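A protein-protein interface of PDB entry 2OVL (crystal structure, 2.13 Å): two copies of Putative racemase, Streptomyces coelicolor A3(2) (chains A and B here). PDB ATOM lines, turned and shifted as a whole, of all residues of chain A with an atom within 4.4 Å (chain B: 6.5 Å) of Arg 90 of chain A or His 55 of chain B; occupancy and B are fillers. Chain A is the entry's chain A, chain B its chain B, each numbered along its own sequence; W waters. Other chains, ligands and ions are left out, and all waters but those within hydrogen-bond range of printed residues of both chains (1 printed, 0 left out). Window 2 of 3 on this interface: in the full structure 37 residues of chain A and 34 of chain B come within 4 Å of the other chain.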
ATOM      1  N   ASP A  67     -18.913  28.788  21.476  1.00  0.00           N
ATOM      2  CA  ASP A  67     -17.697  27.987  21.465  1.00  0.00           C
ATOM      3  C   ASP A  67     -16.453  28.640  20.872  1.00  0.00           C
ATOM      4  O   ASP A  67     -15.414  28.676  21.513  1.00  0.00           O
ATOM      5  CB  ASP A  67     -17.955  26.660  20.740  1.00  0.00           C
ATOM      6  CG  ASP A  67     -19.159  25.909  21.301  1.00  0.00           C
ATOM      7  OD1 ASP A  67     -19.178  25.613  22.519  1.00  0.00           O
ATOM      8  OD2 ASP A  67     -20.088  25.613  20.515  1.00  0.00           O
ATOM      9  N   GLY A  70     -14.391  32.297  22.330  1.00  0.00           N
ATOM     10  CA  GLY A  70     -13.276  32.197  23.258  1.00  0.00           C
ATOM     11  C   GLY A  70     -11.911  31.952  22.632  1.00  0.00           C
ATOM     12  O   GLY A  70     -10.892  32.176  23.280  1.00  0.00           O
ATOM     13  N   CYS A  71     -11.878  31.473  21.390  1.00  0.00           N
ATOM     14  CA  CYS A  71     -10.605  31.235  20.699  1.00  0.00           C
ATOM     15  C   CYS A  71     -10.204  32.510  19.969  1.00  0.00           C
ATOM     16  O   CYS A  71      -9.065  32.657  19.518  1.00  0.00           O
ATOM     17  CB  CYS A  71     -10.741  30.153  19.624  1.00  0.00           C
ATOM     18  SG  CYS A  71     -11.086  28.497  20.178  1.00  0.00           S
ATOM     19  N   SER A  86      -6.865  26.038  16.496  1.00  0.00           N
ATOM     20  CA  SER A  86      -7.443  26.118  17.833  1.00  0.00           C
ATOM     21  C   SER A  86      -8.952  25.874  17.767  1.00  0.00           C
ATOM     22  O   SER A  86      -9.522  25.233  18.647  1.00  0.00           O
ATOM     23  CB  SER A  86      -7.148  27.487  18.470  1.00  0.00           C
ATOM     24  OG  SER A  86      -7.730  28.529  17.714  1.00  0.00           O
ATOM     25  N   MET A  87      -9.596  26.377  16.719  1.00  0.00           N
ATOM     26  CA  MET A  87     -11.037  26.194  16.557  1.00  0.00           C
ATOM     27  C   MET A  87     -11.387  24.754  16.206  1.00  0.00           C
ATOM     28  O   MET A  87     -12.367  24.201  16.715  1.00  0.00           O
ATOM     29  CB  MET A  87     -11.570  27.137  15.483  1.00  0.00           C
ATOM     30  CG  MET A  87     -11.667  28.577  15.961  1.00  0.00           C
ATOM     31  SD  MET A  87     -12.451  29.740  14.652  1.00  0.00           S
ATOM     32  CE  MET A  87     -13.673  28.562  13.827  1.00  0.00           C
ATOM     33  N   TRP A  88     -10.585  24.157  15.330  1.00  0.00           N
ATOM     34  CA  TRP A  88     -10.777  22.770  14.923  1.00  0.00           C
ATOM     35  C   TRP A  88     -10.728  21.886  16.167  1.00  0.00           C
ATOM     36  O   TRP A  88     -11.592  21.031  16.363  1.00  0.00           O
ATOM     37  CB  TRP A  88      -9.682  22.369  13.918  1.00  0.00           C
ATOM     38  CG  TRP A  88      -9.586  20.895  13.597  1.00  0.00           C
ATOM     39  CD1 TRP A  88      -8.653  20.010  14.071  1.00  0.00           C
ATOM     40  CD2 TRP A  88     -10.434  20.146  12.711  1.00  0.00           C
ATOM     41  NE1 TRP A  88      -8.866  18.757  13.529  1.00  0.00           N
ATOM     42  CE2 TRP A  88      -9.952  18.814  12.695  1.00  0.00           C
ATOM     43  CE3 TRP A  88     -11.549  20.470  11.926  1.00  0.00           C
ATOM     44  CZ2 TRP A  88     -10.551  17.807  11.928  1.00  0.00           C
ATOM     45  CZ3 TRP A  88     -12.146  19.465  11.157  1.00  0.00           C
ATOM     46  CH2 TRP A  88     -11.642  18.151  11.167  1.00  0.00           C
ATOM     47  N   TRP A  89      -9.736  22.109  17.026  1.00  0.00           N
ATOM     48  CA  TRP A  89      -9.628  21.307  18.238  1.00  0.00           C
ATOM     49  C   TRP A  89     -10.642  21.672  19.317  1.00  0.00           C
ATOM     50  O   TRP A  89     -11.020  20.833  20.131  1.00  0.00           O
ATOM     51  CB  TRP A  89      -8.197  21.359  18.788  1.00  0.00           C
ATOM     52  CG  TRP A  89      -7.290  20.454  17.993  1.00  0.00           C
ATOM     53  CD1 TRP A  89      -6.378  20.819  17.039  1.00  0.00           C
ATOM     54  CD2 TRP A  89      -7.328  19.021  17.984  1.00  0.00           C
ATOM     55  NE1 TRP A  89      -5.854  19.696  16.430  1.00  0.00           N
ATOM     56  CE2 TRP A  89      -6.419  18.583  16.993  1.00  0.00           C
ATOM     57  CE3 TRP A  89      -8.048  18.065  18.717  1.00  0.00           C
ATOM     58  CZ2 TRP A  89      -6.210  17.225  16.716  1.00  0.00           C
ATOM     59  CZ3 TRP A  89      -7.840  16.718  18.440  1.00  0.00           C
ATOM     60  CH2 TRP A  89      -6.926  16.314  17.446  1.00  0.00           C
ATOM     61  N   ARG A  90     -11.103  22.915  19.317  1.00  0.00           N
ATOM     62  CA  ARG A  90     -12.088  23.319  20.306  1.00  0.00           C
ATOM     63  C   ARG A  90     -13.415  22.569  20.110  1.00  0.00           C
ATOM     64  O   ARG A  90     -14.083  22.210  21.086  1.00  0.00           O
ATOM     65  CB  ARG A  90     -12.326  24.826  20.232  1.00  0.00           C
ATOM     66  CG  ARG A  90     -13.558  25.260  20.981  1.00  0.00           C
ATOM     67  CD  ARG A  90     -13.401  26.654  21.528  1.00  0.00           C
ATOM     68  NE  ARG A  90     -12.357  26.708  22.538  1.00  0.00           N
ATOM     69  CZ  ARG A  90     -12.271  27.657  23.463  1.00  0.00           C
ATOM     70  NH1 ARG A  90     -13.173  28.629  23.500  1.00  0.00           N
ATOM     71  NH2 ARG A  90     -11.291  27.629  24.355  1.00  0.00           N
ATOM     72  N   LEU A  91     -13.798  22.342  18.855  1.00  0.00           N
ATOM     73  CA  LEU A  91     -15.034  21.628  18.556  1.00  0.00           C
ATOM     74  C   LEU A  91     -14.775  20.204  18.056  1.00  0.00           C
ATOM     75  O   LEU A  91     -15.642  19.594  17.425  1.00  0.00           O
ATOM     76  CB  LEU A  91     -15.848  22.393  17.505  1.00  0.00           C
ATOM     77  CG  LEU A  91     -16.533  23.690  17.954  1.00  0.00           C
ATOM     78  CD1 LEU A  91     -17.141  24.403  16.761  1.00  0.00           C
ATOM     79  CD2 LEU A  91     -17.608  23.363  18.992  1.00  0.00           C
ATOM     80  N   HIS A  92     -13.594  19.669  18.346  1.00  0.00           N
ATOM     81  CA  HIS A  92     -13.245  18.327  17.883  1.00  0.00           C
ATOM     82  C   HIS A  92     -14.070  17.220  18.542  1.00  0.00           C
ATOM     83  O   HIS A  92     -14.556  16.305  17.870  1.00  0.00           O
ATOM     84  CB  HIS A  92     -11.753  18.078  18.101  1.00  0.00           C
ATOM     85  CG  HIS A  92     -11.203  16.959  17.274  1.00  0.00           C
ATOM     86  ND1 HIS A  92     -11.279  15.640  17.662  1.00  0.00           N
ATOM     87  CD2 HIS A  92     -10.600  16.960  16.062  1.00  0.00           C
ATOM     88  CE1 HIS A  92     -10.745  14.877  16.726  1.00  0.00           C
ATOM     89  NE2 HIS A  92     -10.326  15.654  15.744  1.00  0.00           N
ATOM     90  N   ARG B  13     -24.515  21.623  32.905  1.00  0.00           N
ATOM     91  CA  ARG B  13     -23.076  21.814  32.973  1.00  0.00           C
ATOM     92  C   ARG B  13     -22.575  21.052  34.173  1.00  0.00           C
ATOM     93  O   ARG B  13     -22.596  21.564  35.289  1.00  0.00           O
ATOM     94  CB  ARG B  13     -22.740  23.290  33.162  1.00  0.00           C
ATOM     95  CG  ARG B  13     -22.375  24.004  31.895  1.00  0.00           C
ATOM     96  CD  ARG B  13     -20.872  24.135  31.754  1.00  0.00           C
ATOM     97  NE  ARG B  13     -20.527  24.761  30.482  1.00  0.00           N
ATOM     98  CZ  ARG B  13     -21.019  25.923  30.065  1.00  0.00           C
ATOM     99  NH1 ARG B  13     -21.880  26.592  30.821  1.00  0.00           N
ATOM    100  NH2 ARG B  13     -20.651  26.415  28.889  1.00  0.00           N
ATOM    101  N   MET B  29     -12.747  20.701  32.071  1.00  0.00           N
ATOM    102  CA  MET B  29     -13.381  21.491  33.111  1.00  0.00           C
ATOM    103  C   MET B  29     -14.783  20.998  33.411  1.00  0.00           C
ATOM    104  O   MET B  29     -15.245  21.066  34.551  1.00  0.00           O
ATOM    105  CB  MET B  29     -13.434  22.952  32.675  1.00  0.00           C
ATOM    106  CG  MET B  29     -12.286  23.333  31.769  1.00  0.00           C
ATOM    107  SD  MET B  29     -12.184  25.214  31.433  1.00  0.00           S
ATOM    108  CE  MET B  29     -10.416  25.519  32.152  1.00  0.00           C
ATOM    109  N   ASP B  30     -15.457  20.490  32.388  1.00  0.00           N
ATOM    110  CA  ASP B  30     -16.813  20.009  32.570  1.00  0.00           C
ATOM    111  C   ASP B  30     -17.340  19.350  31.313  1.00  0.00           C
ATOM    112  O   ASP B  30     -16.838  19.591  30.217  1.00  0.00           O
ATOM    113  CB  ASP B  30     -17.721  21.188  32.921  1.00  0.00           C
ATOM    114  CG  ASP B  30     -17.691  22.287  31.857  1.00  0.00           C
ATOM    115  OD1 ASP B  30     -18.113  22.029  30.707  1.00  0.00           O
ATOM    116  OD2 ASP B  30     -17.240  23.412  32.172  1.00  0.00           O
ATOM    117  N   GLU B  32     -20.790  18.809  29.049  1.00  0.00           N
ATOM    118  CA  GLU B  32     -22.126  19.333  28.840  1.00  0.00           C
ATOM    119  C   GLU B  32     -23.105  18.222  28.489  1.00  0.00           C
ATOM    120  O   GLU B  32     -23.081  17.667  27.387  1.00  0.00           O
ATOM    121  CB  GLU B  32     -22.069  20.402  27.751  1.00  0.00           C
ATOM    122  CG  GLU B  32     -21.006  21.450  28.051  1.00  0.00           C
ATOM    123  CD  GLU B  32     -21.006  22.607  27.078  1.00  0.00           C
ATOM    124  OE1 GLU B  32     -20.697  22.393  25.887  1.00  0.00           O
ATOM    125  OE2 GLU B  32     -21.316  23.736  27.513  1.00  0.00           O
ATOM    126  N   THR B  52     -20.786  16.311  25.793  1.00  0.00           N
ATOM    127  CA  THR B  52     -19.615  16.798  25.084  1.00  0.00           C
ATOM    128  C   THR B  52     -18.651  17.184  26.187  1.00  0.00           C
ATOM    129  O   THR B  52     -19.036  17.293  27.356  1.00  0.00           O
ATOM    130  CB  THR B  52     -19.887  18.058  24.224  1.00  0.00           C
ATOM    131  OG1 THR B  52     -20.290  19.142  25.071  1.00  0.00           O
ATOM    132  CG2 THR B  52     -20.963  17.783  23.183  1.00  0.00           C
ATOM    133  N   VAL B  53     -17.394  17.370  25.822  1.00  0.00           N
ATOM    134  CA  VAL B  53     -16.401  17.776  26.791  1.00  0.00           C
ATOM    135  C   VAL B  53     -16.046  19.239  26.523  1.00  0.00           C
ATOM    136  O   VAL B  53     -15.619  19.588  25.426  1.00  0.00           O
ATOM    137  CB  VAL B  53     -15.148  16.894  26.688  1.00  0.00           C
ATOM    138  CG1 VAL B  53     -14.051  17.441  27.577  1.00  0.00           C
ATOM    139  CG2 VAL B  53     -15.498  15.467  27.095  1.00  0.00           C
ATOM    140  N   ASN B  54     -16.271  20.089  27.519  1.00  0.00           N
ATOM    141  CA  ASN B  54     -15.965  21.518  27.437  1.00  0.00           C
ATOM    142  C   ASN B  54     -16.800  22.384  26.496  1.00  0.00           C
ATOM    143  O   ASN B  54     -17.327  23.413  26.921  1.00  0.00           O
ATOM    144  CB  ASN B  54     -14.478  21.723  27.123  1.00  0.00           C
ATOM    145  CG  ASN B  54     -13.580  21.244  28.245  1.00  0.00           C
ATOM    146  OD1 ASN B  54     -13.928  21.357  29.422  1.00  0.00           O
ATOM    147  ND2 ASN B  54     -12.413  20.718  27.892  1.00  0.00           N
ATOM    148  N   HIS B  55     -16.929  21.995  25.230  1.00  0.00           N
ATOM    149  CA  HIS B  55     -17.707  22.803  24.289  1.00  0.00           C
ATOM    150  C   HIS B  55     -18.635  22.015  23.384  1.00  0.00           C
ATOM    151  O   HIS B  55     -18.524  20.796  23.271  1.00  0.00           O
ATOM    152  CB  HIS B  55     -16.777  23.632  23.398  1.00  0.00           C
ATOM    153  CG  HIS B  55     -15.847  24.517  24.160  1.00  0.00           C
ATOM    154  ND1 HIS B  55     -14.589  24.111  24.552  1.00  0.00           N
ATOM    155  CD2 HIS B  55     -16.010  25.769  24.648  1.00  0.00           C
ATOM    156  CE1 HIS B  55     -14.018  25.074  25.251  1.00  0.00           C
ATOM    157  NE2 HIS B  55     -14.859  26.091  25.325  1.00  0.00           N
ATOM    158  N   GLY B  56     -19.545  22.743  22.738  1.00  0.00           N
ATOM    159  CA  GLY B  56     -20.487  22.148  21.805  1.00  0.00           C
ATOM    160  C   GLY B  56     -21.825  21.695  22.356  1.00  0.00           C
ATOM    161  O   GLY B  56     -22.731  21.371  21.591  1.00  0.00           O
ATOM    162  N   GLY B  57     -21.954  21.670  23.676  1.00  0.00           N
ATOM    163  CA  GLY B  57     -23.196  21.231  24.286  1.00  0.00           C
ATOM    164  C   GLY B  57     -24.436  22.008  23.888  1.00  0.00           C
ATOM    165  O   GLY B  57     -25.455  21.415  23.513  1.00  0.00           O
ATOM    166  N   ALA B  58     -24.359  23.333  23.973  1.00  0.00           N
ATOM    167  CA  ALA B  58     -25.486  24.184  23.625  1.00  0.00           C
ATOM    168  C   ALA B  58     -25.904  23.939  22.180  1.00  0.00           C
ATOM    169  O   ALA B  58     -27.094  23.947  21.853  1.00  0.00           O
ATOM    170  CB  ALA B  58     -25.114  25.656  23.831  1.00  0.00           C
ATOM    171  N   HIS B  99     -21.527  17.066  15.351  1.00  0.00           N
ATOM    172  CA  HIS B  99     -22.430  17.178  16.491  1.00  0.00           C
ATOM    173  C   HIS B  99     -23.848  16.691  16.237  1.00  0.00           C
ATOM    174  O   HIS B  99     -24.501  16.194  17.145  1.00  0.00           O
ATOM    175  CB  HIS B  99     -22.447  18.629  16.993  1.00  0.00           C
ATOM    176  CG  HIS B  99     -21.136  19.072  17.560  1.00  0.00           C
ATOM    177  ND1 HIS B  99     -20.034  19.323  16.773  1.00  0.00           N
ATOM    178  CD2 HIS B  99     -20.727  19.232  18.841  1.00  0.00           C
ATOM    179  CE1 HIS B  99     -19.000  19.613  17.543  1.00  0.00           C
ATOM    180  NE2 HIS B  99     -19.394  19.563  18.802  1.00  0.00           N
HETATM  181  O   HOH W   1     -22.299  24.907  21.907  1.00  0.00           O
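Among the printed residues, merely in contact across the chains: Asp 67 of chain A with His 55 of chain B (3.2 Å), Arg 90 of chain A with His 55 of chain B (3.6 Å) and Leu 91 of chain A with His 99 of chain B (3.4 Å).
The backbone NH (N) of Gly 56 of chain B sits at hydrogen-bond distance from the side-chain carboxylate (OD1) of Asp 67 of chain A (2.9 Å).
NH1 of Arg 90 of chain A lies close to O of Asp 67 of chain A (3.0 Å). The side-chain sulfur (SG) of Cys 71 of chain A lies within hydrogen-bond range of the guanidinium group (NE) of Arg 90 of chain A (3.2 Å). OE1 of Glu 32 of chain B lies within hydrogen-bond range of N of Gly 56 of chain B, 3.4 Å away. OG1 of Thr 52 of chain B lies within hydrogen-bond range of O of His 55 of chain B.
Hydrophobic or aromatic side chains of chain B that line the printed part of chain A: His 55 and His 99.
Water W1 bridges OD2 of Asp 67 of chain A and N of Ala 58 of chain B.
Arg 90 of chain A touches just one residue of chain B: His 55 (3.6 Å). Of chain A, only Asp 67 and Arg 90 come within 4 Å of His 55 of chain B. Of the printed residues of chain B, Asp 67 of chain A touches His 55 and Gly 56. Of the printed residues of chain A, Gly 56 of chain B touches Asp 67. Of the printed residues of chain B, Leu 91 of chain A touches His 99. Of the printed residues of chain A, His 99 of chain B touches Leu 91. Val 53 of chain B touches none of the printed residues of chain A. Met 87 of chain A touches none of the printed residues of chain B. The nearest residue of chain B that does not touch Arg 90 of chain A is Val 53 of chain B (5.3 Å). The nearest printed residue of chain B that does not touch Leu 91 of chain A is Gly 56 of chain B (4.2 Å).
No position is printed for both chains. Of the 4 pairs that touch across the chains among the printed residues, none has its exchanged pair printed and touching as well.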
